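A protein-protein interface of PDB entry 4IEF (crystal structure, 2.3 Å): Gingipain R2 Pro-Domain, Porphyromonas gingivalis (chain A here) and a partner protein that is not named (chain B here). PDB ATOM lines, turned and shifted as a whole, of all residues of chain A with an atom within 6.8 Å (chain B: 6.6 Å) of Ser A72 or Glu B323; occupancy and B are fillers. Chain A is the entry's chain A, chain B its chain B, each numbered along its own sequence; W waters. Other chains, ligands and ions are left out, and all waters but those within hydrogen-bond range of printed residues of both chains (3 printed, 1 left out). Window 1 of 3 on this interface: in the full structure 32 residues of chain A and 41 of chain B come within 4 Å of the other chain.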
ATOM      1  N   GLU A  54     -36.819 -12.058  -3.210  1.00  0.00           N
ATOM      2  CA  GLU A  54     -35.436 -11.570  -3.313  1.00  0.00           C
ATOM      3  C   GLU A  54     -35.215 -10.280  -2.472  1.00  0.00           C
ATOM      4  O   GLU A  54     -34.173  -9.625  -2.597  1.00  0.00           O
ATOM      5  CB  GLU A  54     -35.039 -11.360  -4.790  1.00  0.00           C
ATOM      6  CG  GLU A  54     -33.588 -11.661  -5.107  1.00  0.00           C
ATOM      7  CD  GLU A  54     -33.164 -11.326  -6.523  1.00  0.00           C
ATOM      8  OE1 GLU A  54     -34.001 -11.444  -7.448  1.00  0.00           O
ATOM      9  OE2 GLU A  54     -31.983 -10.958  -6.710  1.00  0.00           O
ATOM     10  N   ILE A  68     -34.809  -4.383   0.551  1.00  0.00           N
ATOM     11  CA  ILE A  68     -34.288  -3.945  -0.735  1.00  0.00           C
ATOM     12  C   ILE A  68     -34.005  -5.157  -1.638  1.00  0.00           C
ATOM     13  O   ILE A  68     -33.906  -6.288  -1.157  1.00  0.00           O
ATOM     14  CB  ILE A  68     -33.008  -3.063  -0.561  1.00  0.00           C
ATOM     15  CG1 ILE A  68     -31.797  -3.872  -0.029  1.00  0.00           C
ATOM     16  CG2 ILE A  68     -33.288  -1.778   0.266  1.00  0.00           C
ATOM     17  CD1 ILE A  68     -30.426  -3.319  -0.480  1.00  0.00           C
ATOM     18  N   LEU A  69     -33.875  -4.908  -2.936  1.00  0.00           N
ATOM     19  CA  LEU A  69     -33.503  -5.920  -3.913  1.00  0.00           C
ATOM     20  C   LEU A  69     -32.213  -5.452  -4.570  1.00  0.00           C
ATOM     21  O   LEU A  69     -32.142  -4.321  -5.054  1.00  0.00           O
ATOM     22  CB  LEU A  69     -34.615  -6.177  -4.942  1.00  0.00           C
ATOM     23  CG  LEU A  69     -34.413  -7.404  -5.825  1.00  0.00           C
ATOM     24  CD1 LEU A  69     -35.724  -8.069  -6.100  1.00  0.00           C
ATOM     25  CD2 LEU A  69     -33.691  -7.047  -7.132  1.00  0.00           C
ATOM     26  N   SER A  70     -31.196  -6.315  -4.571  1.00  0.00           N
ATOM     27  CA  SER A  70     -29.881  -5.983  -5.117  1.00  0.00           C
ATOM     28  C   SER A  70     -29.497  -6.885  -6.279  1.00  0.00           C
ATOM     29  O   SER A  70     -29.762  -8.091  -6.249  1.00  0.00           O
ATOM     30  CB  SER A  70     -28.821  -6.072  -4.027  1.00  0.00           C
ATOM     31  OG  SER A  70     -29.069  -5.147  -2.980  1.00  0.00           O
ATOM     32  N   ARG A  71     -28.890  -6.274  -7.317  1.00  0.00           N
ATOM     33  CA  ARG A  71     -28.420  -6.950  -8.521  1.00  0.00           C
ATOM     34  C   ARG A  71     -27.075  -6.391  -8.954  1.00  0.00           C
ATOM     35  O   ARG A  71     -26.847  -5.178  -8.891  1.00  0.00           O
ATOM     36  CB  ARG A  71     -29.444  -6.837  -9.672  1.00  0.00           C
ATOM     37  CG  ARG A  71     -30.660  -7.750  -9.542  1.00  0.00           C
ATOM     38  CD  ARG A  71     -30.306  -9.231  -9.587  1.00  0.00           C
ATOM     39  NE  ARG A  71     -31.495 -10.066  -9.410  1.00  0.00           N
ATOM     40  CZ  ARG A  71     -32.236 -10.540 -10.406  1.00  0.00           C
ATOM     41  NH1 ARG A  71     -31.906 -10.290 -11.667  1.00  0.00           N
ATOM     42  NH2 ARG A  71     -33.308 -11.280 -10.149  1.00  0.00           N
ATOM     43  N   SER A  72     -26.194  -7.283  -9.408  1.00  0.00           N
ATOM     44  CA  SER A  72     -24.844  -6.937  -9.842  1.00  0.00           C
ATOM     45  C   SER A  72     -24.799  -6.662 -11.330  1.00  0.00           C
ATOM     46  O   SER A  72     -25.441  -7.365 -12.122  1.00  0.00           O
ATOM     47  CB  SER A  72     -23.863  -8.047  -9.480  1.00  0.00           C
ATOM     48  OG  SER A  72     -23.823  -8.243  -8.076  1.00  0.00           O
ATOM     49  N   LEU A  73     -24.031  -5.635 -11.707  1.00  0.00           N
ATOM     50  CA  LEU A  73     -23.859  -5.258 -13.099  1.00  0.00           C
ATOM     51  C   LEU A  73     -22.396  -5.100 -13.456  1.00  0.00           C
ATOM     52  O   LEU A  73     -21.615  -4.580 -12.654  1.00  0.00           O
ATOM     53  CB  LEU A  73     -24.589  -3.935 -13.416  1.00  0.00           C
ATOM     54  CG  LEU A  73     -26.121  -3.899 -13.317  1.00  0.00           C
ATOM     55  CD1 LEU A  73     -26.614  -2.462 -13.229  1.00  0.00           C
ATOM     56  CD2 LEU A  73     -26.778  -4.627 -14.498  1.00  0.00           C
ATOM     57  N   ALA A  74     -22.027  -5.555 -14.665  1.00  0.00           N
ATOM     58  CA  ALA A  74     -20.706  -5.327 -15.244  1.00  0.00           C
ATOM     59  C   ALA A  74     -20.714  -3.852 -15.706  1.00  0.00           C
ATOM     60  O   ALA A  74     -21.570  -3.476 -16.514  1.00  0.00           O
ATOM     61  CB  ALA A  74     -20.457  -6.294 -16.400  1.00  0.00           C
ATOM     62  N   SER A 136     -24.014   0.438  -4.820  1.00  0.00           N
ATOM     63  CA  SER A 136     -23.052   0.035  -3.801  1.00  0.00           C
ATOM     64  C   SER A 136     -21.642   0.357  -4.334  1.00  0.00           C
ATOM     65  O   SER A 136     -21.513   0.721  -5.502  1.00  0.00           O
ATOM     66  CB  SER A 136     -23.217  -1.440  -3.447  1.00  0.00           C
ATOM     67  OG  SER A 136     -24.389  -1.638  -2.671  1.00  0.00           O
ATOM     68  N   PHE A 139     -16.541  -2.774  -7.433  1.00  0.00           N
ATOM     69  CA  PHE A 139     -15.605  -3.855  -7.149  1.00  0.00           C
ATOM     70  C   PHE A 139     -14.974  -4.373  -8.433  1.00  0.00           C
ATOM     71  O   PHE A 139     -15.492  -4.123  -9.519  1.00  0.00           O
ATOM     72  CB  PHE A 139     -16.328  -4.999  -6.404  1.00  0.00           C
ATOM     73  CG  PHE A 139     -17.441  -5.691  -7.161  1.00  0.00           C
ATOM     74  CD1 PHE A 139     -17.182  -6.810  -7.941  1.00  0.00           C
ATOM     75  CD2 PHE A 139     -18.761  -5.259  -7.043  1.00  0.00           C
ATOM     76  CE1 PHE A 139     -18.217  -7.464  -8.620  1.00  0.00           C
ATOM     77  CE2 PHE A 139     -19.795  -5.914  -7.724  1.00  0.00           C
ATOM     78  CZ  PHE A 139     -19.517  -7.010  -8.509  1.00  0.00           C
ATOM     79  N   GLY A 146     -17.290  -4.410 -11.528  1.00  0.00           N
ATOM     80  CA  GLY A 146     -18.709  -4.539 -11.237  1.00  0.00           C
ATOM     81  C   GLY A 146     -19.221  -3.534 -10.231  1.00  0.00           C
ATOM     82  O   GLY A 146     -18.440  -2.915  -9.495  1.00  0.00           O
ATOM     83  N   GLN A 147     -20.547  -3.368 -10.204  1.00  0.00           N
ATOM     84  CA  GLN A 147     -21.241  -2.489  -9.269  1.00  0.00           C
ATOM     85  C   GLN A 147     -22.664  -3.007  -9.044  1.00  0.00           C
ATOM     86  O   GLN A 147     -23.333  -3.428  -9.993  1.00  0.00           O
ATOM     87  CB  GLN A 147     -21.236  -1.025  -9.738  1.00  0.00           C
ATOM     88  CG  GLN A 147     -21.391  -0.054  -8.567  1.00  0.00           C
ATOM     89  CD  GLN A 147     -21.000   1.369  -8.861  1.00  0.00           C
ATOM     90  OE1 GLN A 147     -20.613   1.725  -9.971  1.00  0.00           O
ATOM     91  NE2 GLN A 147     -21.092   2.224  -7.854  1.00  0.00           N
ATOM     92  N   VAL A 148     -23.112  -2.987  -7.781  1.00  0.00           N
ATOM     93  CA  VAL A 148     -24.438  -3.470  -7.403  1.00  0.00           C
ATOM     94  C   VAL A 148     -25.435  -2.309  -7.361  1.00  0.00           C
ATOM     95  O   VAL A 148     -25.172  -1.287  -6.722  1.00  0.00           O
ATOM     96  CB  VAL A 148     -24.403  -4.248  -6.060  1.00  0.00           C
ATOM     97  CG1 VAL A 148     -25.805  -4.684  -5.626  1.00  0.00           C
ATOM     98  CG2 VAL A 148     -23.469  -5.455  -6.150  1.00  0.00           C
ATOM     99  N   VAL A 149     -26.577  -2.480  -8.053  1.00  0.00           N
ATOM    100  CA  VAL A 149     -27.682  -1.523  -8.040  1.00  0.00           C
ATOM    101  C   VAL A 149     -28.726  -2.035  -7.011  1.00  0.00           C
ATOM    102  O   VAL A 149     -29.058  -3.222  -7.002  1.00  0.00           O
ATOM    103  CB  VAL A 149     -28.285  -1.215  -9.452  1.00  0.00           C
ATOM    104  CG1 VAL A 149     -28.900  -2.448 -10.118  1.00  0.00           C
ATOM    105  CG2 VAL A 149     -29.291  -0.065  -9.389  1.00  0.00           C
ATOM    106  N   ASN A 150     -29.186  -1.149  -6.118  1.00  0.00           N
ATOM    107  CA  ASN A 150     -30.173  -1.492  -5.089  1.00  0.00           C
ATOM    108  C   ASN A 150     -31.496  -0.769  -5.310  1.00  0.00           C
ATOM    109  O   ASN A 150     -31.528   0.457  -5.453  1.00  0.00           O
ATOM    110  CB  ASN A 150     -29.641  -1.159  -3.687  1.00  0.00           C
ATOM    111  CG  ASN A 150     -28.194  -1.531  -3.504  1.00  0.00           C
ATOM    112  OD1 ASN A 150     -27.827  -2.707  -3.564  1.00  0.00           O
ATOM    113  ND2 ASN A 150     -27.333  -0.530  -3.374  1.00  0.00           N
ATOM    114  N   SER A 201     -23.001 -15.527 -14.465  1.00  0.00           N
ATOM    115  CA  SER A 201     -23.865 -15.803 -13.316  1.00  0.00           C
ATOM    116  C   SER A 201     -23.901 -14.646 -12.311  1.00  0.00           C
ATOM    117  O   SER A 201     -24.929 -14.452 -11.671  1.00  0.00           O
ATOM    118  CB  SER A 201     -23.435 -17.086 -12.614  1.00  0.00           C
ATOM    119  OG  SER A 201     -22.081 -17.026 -12.198  1.00  0.00           O
ATOM    120  N   VAL A 202     -22.794 -13.899 -12.153  1.00  0.00           N
ATOM    121  CA  VAL A 202     -22.720 -12.772 -11.218  1.00  0.00           C
ATOM    122  C   VAL A 202     -23.417 -11.541 -11.837  1.00  0.00           C
ATOM    123  O   VAL A 202     -24.273 -10.949 -11.187  1.00  0.00           O
ATOM    124  CB  VAL A 202     -21.251 -12.471 -10.784  1.00  0.00           C
ATOM    125  CG1 VAL A 202     -21.116 -11.105 -10.116  1.00  0.00           C
ATOM    126  CG2 VAL A 202     -20.713 -13.559  -9.862  1.00  0.00           C
ATOM    127  N   PHE A 203     -23.050 -11.165 -13.077  1.00  0.00           N
ATOM    128  CA  PHE A 203     -23.587  -9.981 -13.751  1.00  0.00           C
ATOM    129  C   PHE A 203     -24.756 -10.341 -14.667  1.00  0.00           C
ATOM    130  O   PHE A 203     -24.625 -11.209 -15.531  1.00  0.00           O
ATOM    131  CB  PHE A 203     -22.480  -9.249 -14.533  1.00  0.00           C
ATOM    132  CG  PHE A 203     -21.208  -9.016 -13.748  1.00  0.00           C
ATOM    133  CD1 PHE A 203     -20.039  -9.694 -14.071  1.00  0.00           C
ATOM    134  CD2 PHE A 203     -21.188  -8.146 -12.660  1.00  0.00           C
ATOM    135  CE1 PHE A 203     -18.869  -9.494 -13.333  1.00  0.00           C
ATOM    136  CE2 PHE A 203     -20.013  -7.933 -11.934  1.00  0.00           C
ATOM    137  CZ  PHE A 203     -18.859  -8.605 -12.278  1.00  0.00           C
ATOM    138  N   MET A 204     -25.903  -9.665 -14.470  1.00  0.00           N
ATOM    139  CA  MET A 204     -27.111  -9.909 -15.268  1.00  0.00           C
ATOM    140  C   MET A 204     -27.040  -9.233 -16.665  1.00  0.00           C
ATOM    141  O   MET A 204     -27.881  -9.522 -17.518  1.00  0.00           O
ATOM    142  CB  MET A 204     -28.398  -9.499 -14.506  1.00  0.00           C
ATOM    143  CG  MET A 204     -28.539  -8.008 -14.185  1.00  0.00           C
ATOM    144  SD  MET A 204     -30.063  -7.611 -13.251  1.00  0.00           S
ATOM    145  CE  MET A 204     -31.316  -7.895 -14.501  1.00  0.00           C
ATOM    146  N   ASN A 205     -26.010  -8.397 -16.913  1.00  0.00           N
ATOM    147  CA  ASN A 205     -25.820  -7.697 -18.184  1.00  0.00           C
ATOM    148  C   ASN A 205     -24.554  -8.164 -18.946  1.00  0.00           C
ATOM    149  O   ASN A 205     -24.240  -7.588 -19.995  1.00  0.00           O
ATOM    150  CB  ASN A 205     -25.743  -6.179 -17.935  1.00  0.00           C
ATOM    151  CG  ASN A 205     -24.486  -5.729 -17.230  1.00  0.00           C
ATOM    152  OD1 ASN A 205     -24.040  -6.331 -16.248  1.00  0.00           O
ATOM    153  ND2 ASN A 205     -23.868  -4.679 -17.737  1.00  0.00           N
ATOM    154  N   TYR A 206     -23.851  -9.206 -18.444  1.00  0.00           N
ATOM    155  CA  TYR A 206     -22.606  -9.704 -19.044  1.00  0.00           C
ATOM    156  C   TYR A 206     -22.811 -10.336 -20.432  1.00  0.00           C
ATOM    157  O   TYR A 206     -22.090  -9.964 -21.365  1.00  0.00           O
ATOM    158  CB  TYR A 206     -21.873 -10.693 -18.115  1.00  0.00           C
ATOM    159  CG  TYR A 206     -20.486 -11.048 -18.613  1.00  0.00           C
ATOM    160  CD1 TYR A 206     -19.430 -10.146 -18.504  1.00  0.00           C
ATOM    161  CD2 TYR A 206     -20.238 -12.270 -19.234  1.00  0.00           C
ATOM    162  CE1 TYR A 206     -18.162 -10.453 -18.992  1.00  0.00           C
ATOM    163  CE2 TYR A 206     -18.973 -12.588 -19.725  1.00  0.00           C
ATOM    164  CZ  TYR A 206     -17.936 -11.679 -19.598  1.00  0.00           C
ATOM    165  OH  TYR A 206     -16.686 -11.985 -20.079  1.00  0.00           O
ATOM    166  N   TYR B 105     -14.124  -9.332  -3.464  1.00  0.00           N
ATOM    167  CA  TYR B 105     -14.385 -10.302  -4.528  1.00  0.00           C
ATOM    168  C   TYR B 105     -13.075 -10.976  -4.905  1.00  0.00           C
ATOM    169  O   TYR B 105     -12.201 -10.359  -5.529  1.00  0.00           O
ATOM    170  CB  TYR B 105     -15.042  -9.638  -5.747  1.00  0.00           C
ATOM    171  CG  TYR B 105     -16.513  -9.342  -5.559  1.00  0.00           C
ATOM    172  CD1 TYR B 105     -17.488 -10.173  -6.112  1.00  0.00           C
ATOM    173  CD2 TYR B 105     -16.934  -8.226  -4.839  1.00  0.00           C
ATOM    174  CE1 TYR B 105     -18.846  -9.891  -5.968  1.00  0.00           C
ATOM    175  CE2 TYR B 105     -18.291  -7.937  -4.686  1.00  0.00           C
ATOM    176  CZ  TYR B 105     -19.243  -8.773  -5.253  1.00  0.00           C
ATOM    177  OH  TYR B 105     -20.580  -8.497  -5.104  1.00  0.00           O
ATOM    178  N   MET B 318     -20.710 -17.153  -1.776  1.00  0.00           N
ATOM    179  CA  MET B 318     -20.423 -16.008  -0.911  1.00  0.00           C
ATOM    180  C   MET B 318     -20.475 -14.671  -1.669  1.00  0.00           C
ATOM    181  O   MET B 318     -20.606 -13.631  -1.023  1.00  0.00           O
ATOM    182  CB  MET B 318     -19.064 -16.182  -0.215  1.00  0.00           C
ATOM    183  CG  MET B 318     -19.077 -17.315   0.795  1.00  0.00           C
ATOM    184  SD  MET B 318     -17.715 -17.333   1.954  1.00  0.00           S
ATOM    185  CE  MET B 318     -16.366 -17.777   0.883  1.00  0.00           C
ATOM    186  N   PHE B 319     -20.386 -14.691  -3.019  1.00  0.00           N
ATOM    187  CA  PHE B 319     -20.476 -13.476  -3.850  1.00  0.00           C
ATOM    188  C   PHE B 319     -21.868 -12.854  -3.742  1.00  0.00           C
ATOM    189  O   PHE B 319     -21.981 -11.629  -3.640  1.00  0.00           O
ATOM    190  CB  PHE B 319     -20.135 -13.770  -5.320  1.00  0.00           C
ATOM    191  CG  PHE B 319     -18.668 -13.970  -5.640  1.00  0.00           C
ATOM    192  CD1 PHE B 319     -17.676 -13.537  -4.758  1.00  0.00           C
ATOM    193  CD2 PHE B 319     -18.275 -14.549  -6.842  1.00  0.00           C
ATOM    194  CE1 PHE B 319     -16.326 -13.689  -5.072  1.00  0.00           C
ATOM    195  CE2 PHE B 319     -16.923 -14.714  -7.144  1.00  0.00           C
ATOM    196  CZ  PHE B 319     -15.960 -14.284  -6.257  1.00  0.00           C
ATOM    197  N   ALA B 320     -22.923 -13.707  -3.726  1.00  0.00           N
ATOM    198  CA  ALA B 320     -24.330 -13.312  -3.579  1.00  0.00           C
ATOM    199  C   ALA B 320     -24.569 -12.658  -2.219  1.00  0.00           C
ATOM    200  O   ALA B 320     -25.365 -11.736  -2.111  1.00  0.00           O
ATOM    201  CB  ALA B 320     -25.231 -14.527  -3.732  1.00  0.00           C
ATOM    202  N   MET B 321     -23.844 -13.133  -1.199  1.00  0.00           N
ATOM    203  CA  MET B 321     -23.884 -12.647   0.174  1.00  0.00           C
ATOM    204  C   MET B 321     -23.378 -11.185   0.236  1.00  0.00           C
ATOM    205  O   MET B 321     -23.958 -10.384   0.964  1.00  0.00           O
ATOM    206  CB  MET B 321     -23.041 -13.600   1.036  1.00  0.00           C
ATOM    207  CG  MET B 321     -23.059 -13.338   2.511  1.00  0.00           C
ATOM    208  SD  MET B 321     -22.283 -14.727   3.375  1.00  0.00           S
ATOM    209  CE  MET B 321     -20.581 -14.498   2.901  1.00  0.00           C
ATOM    210  N   VAL B 322     -22.342 -10.834  -0.558  1.00  0.00           N
ATOM    211  CA  VAL B 322     -21.806  -9.467  -0.619  1.00  0.00           C
ATOM    212  C   VAL B 322     -22.789  -8.585  -1.415  1.00  0.00           C
ATOM    213  O   VAL B 322     -23.068  -7.451  -1.015  1.00  0.00           O
ATOM    214  CB  VAL B 322     -20.371  -9.428  -1.211  1.00  0.00           C
ATOM    215  CG1 VAL B 322     -19.891  -7.991  -1.433  1.00  0.00           C
ATOM    216  CG2 VAL B 322     -19.394 -10.181  -0.315  1.00  0.00           C
ATOM    217  N   GLU B 323     -23.317  -9.125  -2.530  1.00  0.00           N
ATOM    218  CA  GLU B 323     -24.290  -8.454  -3.388  1.00  0.00           C
ATOM    219  C   GLU B 323     -25.532  -8.028  -2.589  1.00  0.00           C
ATOM    220  O   GLU B 323     -26.017  -6.909  -2.750  1.00  0.00           O
ATOM    221  CB  GLU B 323     -24.702  -9.400  -4.537  1.00  0.00           C
ATOM    222  CG  GLU B 323     -25.819  -8.869  -5.422  1.00  0.00           C
ATOM    223  CD  GLU B 323     -26.391  -9.901  -6.370  1.00  0.00           C
ATOM    224  OE1 GLU B 323     -25.855 -10.040  -7.493  1.00  0.00           O
ATOM    225  OE2 GLU B 323     -27.384 -10.562  -5.996  1.00  0.00           O
ATOM    226  N   LYS B 324     -26.027  -8.914  -1.719  1.00  0.00           N
ATOM    227  CA  LYS B 324     -27.265  -8.702  -0.974  1.00  0.00           C
ATOM    228  C   LYS B 324     -27.090  -8.138   0.449  1.00  0.00           C
ATOM    229  O   LYS B 324     -27.991  -7.416   0.887  1.00  0.00           O
ATOM    230  CB  LYS B 324     -28.071 -10.012  -0.922  1.00  0.00           C
ATOM    231  CG  LYS B 324     -28.327 -10.567  -2.321  1.00  0.00           C
ATOM    232  CD  LYS B 324     -29.650 -11.264  -2.481  1.00  0.00           C
ATOM    233  CE  LYS B 324     -29.854 -11.690  -3.916  1.00  0.00           C
ATOM    234  NZ  LYS B 324     -29.955 -10.526  -4.843  1.00  0.00           N
ATOM    235  N   TYR B 325     -25.973  -8.441   1.165  1.00  0.00           N
ATOM    236  CA  TYR B 325     -25.797  -7.983   2.557  1.00  0.00           C
ATOM    237  C   TYR B 325     -24.647  -6.974   2.779  1.00  0.00           C
ATOM    238  O   TYR B 325     -24.464  -6.505   3.905  1.00  0.00           O
ATOM    239  CB  TYR B 325     -25.648  -9.181   3.493  1.00  0.00           C
ATOM    240  CG  TYR B 325     -26.969  -9.887   3.719  1.00  0.00           C
ATOM    241  CD1 TYR B 325     -27.812  -9.512   4.759  1.00  0.00           C
ATOM    242  CD2 TYR B 325     -27.381 -10.923   2.883  1.00  0.00           C
ATOM    243  CE1 TYR B 325     -29.025 -10.161   4.974  1.00  0.00           C
ATOM    244  CE2 TYR B 325     -28.596 -11.573   3.083  1.00  0.00           C
ATOM    245  CZ  TYR B 325     -29.415 -11.190   4.131  1.00  0.00           C
ATOM    246  OH  TYR B 325     -30.620 -11.824   4.328  1.00  0.00           O
ATOM    247  N   LYS B 326     -23.943  -6.589   1.701  1.00  0.00           N
ATOM    248  CA  LYS B 326     -22.888  -5.564   1.637  1.00  0.00           C
ATOM    249  C   LYS B 326     -21.744  -5.804   2.640  1.00  0.00           C
ATOM    250  O   LYS B 326     -21.165  -6.886   2.631  1.00  0.00           O
ATOM    251  CB  LYS B 326     -23.469  -4.130   1.797  1.00  0.00           C
ATOM    252  CG  LYS B 326     -24.842  -3.881   1.169  1.00  0.00           C
ATOM    253  CD  LYS B 326     -24.837  -3.965  -0.340  1.00  0.00           C
ATOM    254  CE  LYS B 326     -26.230  -3.993  -0.903  1.00  0.00           C
ATOM    255  NZ  LYS B 326     -26.199  -4.235  -2.357  1.00  0.00           N
HETATM  256  O   HOH W   1     -30.079  -7.111  -1.128  1.00  0.00           O
HETATM  257  O   HOH W   2     -26.707  -9.795 -10.313  1.00  0.00           O
HETATM  258  O   HOH W   3     -31.551  -8.367  -2.683  1.00  0.00           O
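The side-chain carboxylate of Glu A54 is in salt-bridge range of the side-chain amino group of Lys B324.
The side-chain amino group of Lys B326 lies within hydrogen-bond range of the side-chain hydroxyl of Ser A70, at 3.1 Å.
The side-chain carboxylate of Glu B323 sits at hydrogen-bond distance from the side-chain hydroxyl of Ser A72 (2.8 Å).
OG of Ser A136 is in hydrogen-bond range of NZ of Lys B326, 3.2 Å away.
O of Ser A70 sits close to OE2 of Glu B323 (3.4 Å).
OD1 of Asn A150 sits at hydrogen-bond distance from NZ of Lys B326 (2.5 Å).
O of Ser A70 lies within hydrogen-bond range of NZ of Lys B324, 2.8 Å away.
The backbone carbonyl oxygen of Val A148 is in hydrogen-bond range of the backbone NH of Ser A136 (2.8 Å).
OD1 of Asn A150 lies within hydrogen-bond range of OG of Ser A70, 2.8 Å away.
The guanidinium group of Arg A71 lies within salt-bridge range of the side-chain carboxylate of Glu A54.
N of Met A204 lies within hydrogen-bond range of O of Ser A72, at 3.3 Å.
OE2 of Glu B323 lies within salt-bridge range of NZ of Lys B324 (2.8 Å).
The backbone carbonyl oxygen of Ser A136 sits at hydrogen-bond distance from the side-chain amide nitrogen of Gln A147 (2.8 Å).
Of the printed residues of chain B, Glu A54 touches Lys B324 (2.8 Å).
Of the printed residues of chain B, Ser A72 touches Glu B323.
Of the printed residues of chain B, Phe A139 touches Tyr B105 (3.4 Å).
Of the printed residues of chain B, Val A148 touches Glu B323 (3.6 Å) and Lys B326 (3.3 Å).
Glu B323 touches just these residues of chain A: Ser A70, Ser A72 and Val A148.
Tyr B325 touches none of the printed residues of chain A.
The nearest printed residue of chain A that does not touch Glu B323 is Arg A71 (4.1 Å).
The nearest printed residue of chain B that does not touch Ser A70 is Tyr B325 (6.1 Å).
Phe A139 touches Tyr B105 (CD1 to CD2, 3.4 Å).
Val A148 touches Glu B323 (CG1 to O, 3.6 Å).
NZ of Lys B326 touches CG1 of Val A148 (3.3 Å).
Water W2 lies within hydrogen-bond range of the backbone NH of Ser A72, the backbone carbonyl oxygen of Val A202 and the side-chain carboxylate of Glu B323.
Water W3 lies within hydrogen-bond range of the backbone NH (N) of Ser A70 (2.8 Å), the backbone carbonyl oxygen (O) of Glu A54 (2.9 Å), the side-chain amino group (NZ) of Lys B324 (3.4 Å) and the backbone carbonyl oxygen (O) of Ile A68 (3.5 Å).
Water W1 lies within hydrogen-bond range of the side-chain hydroxyl of Ser A70 (2.9 Å) and the backbone carbonyl oxygen of Lys B324 (2.9 Å).
Of the 10 printed residues of chain B, 4 touch a printed residue of chain A.
Printed residues of chain B that touch a printed residue of chain A: Tyr B105, Glu B323, Lys B324 and Lys B326.
Hydrophobic or aromatic side chains of chain B that line the printed part of chain A: Tyr B105.
Along chain B the printed residues that touch a printed residue of chain A span positions 105 to 326.
Printed residues of chain A that touch a printed residue of chain B: Glu A54, Ser A70, Ser A72, Ser A136, Phe A139, Val A148 and Asn A150.
Along chain A the printed residues that touch a printed residue of chain B span positions 54 to 150.
Among the printed residues, 10 pairs touch across the chains.
Among the printed residues, Asp or Glu carboxylates within 4 Å of a Lys or Arg side-chain nitrogen of the other chain: Glu A54 with Lys B324 (2.8 Å).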
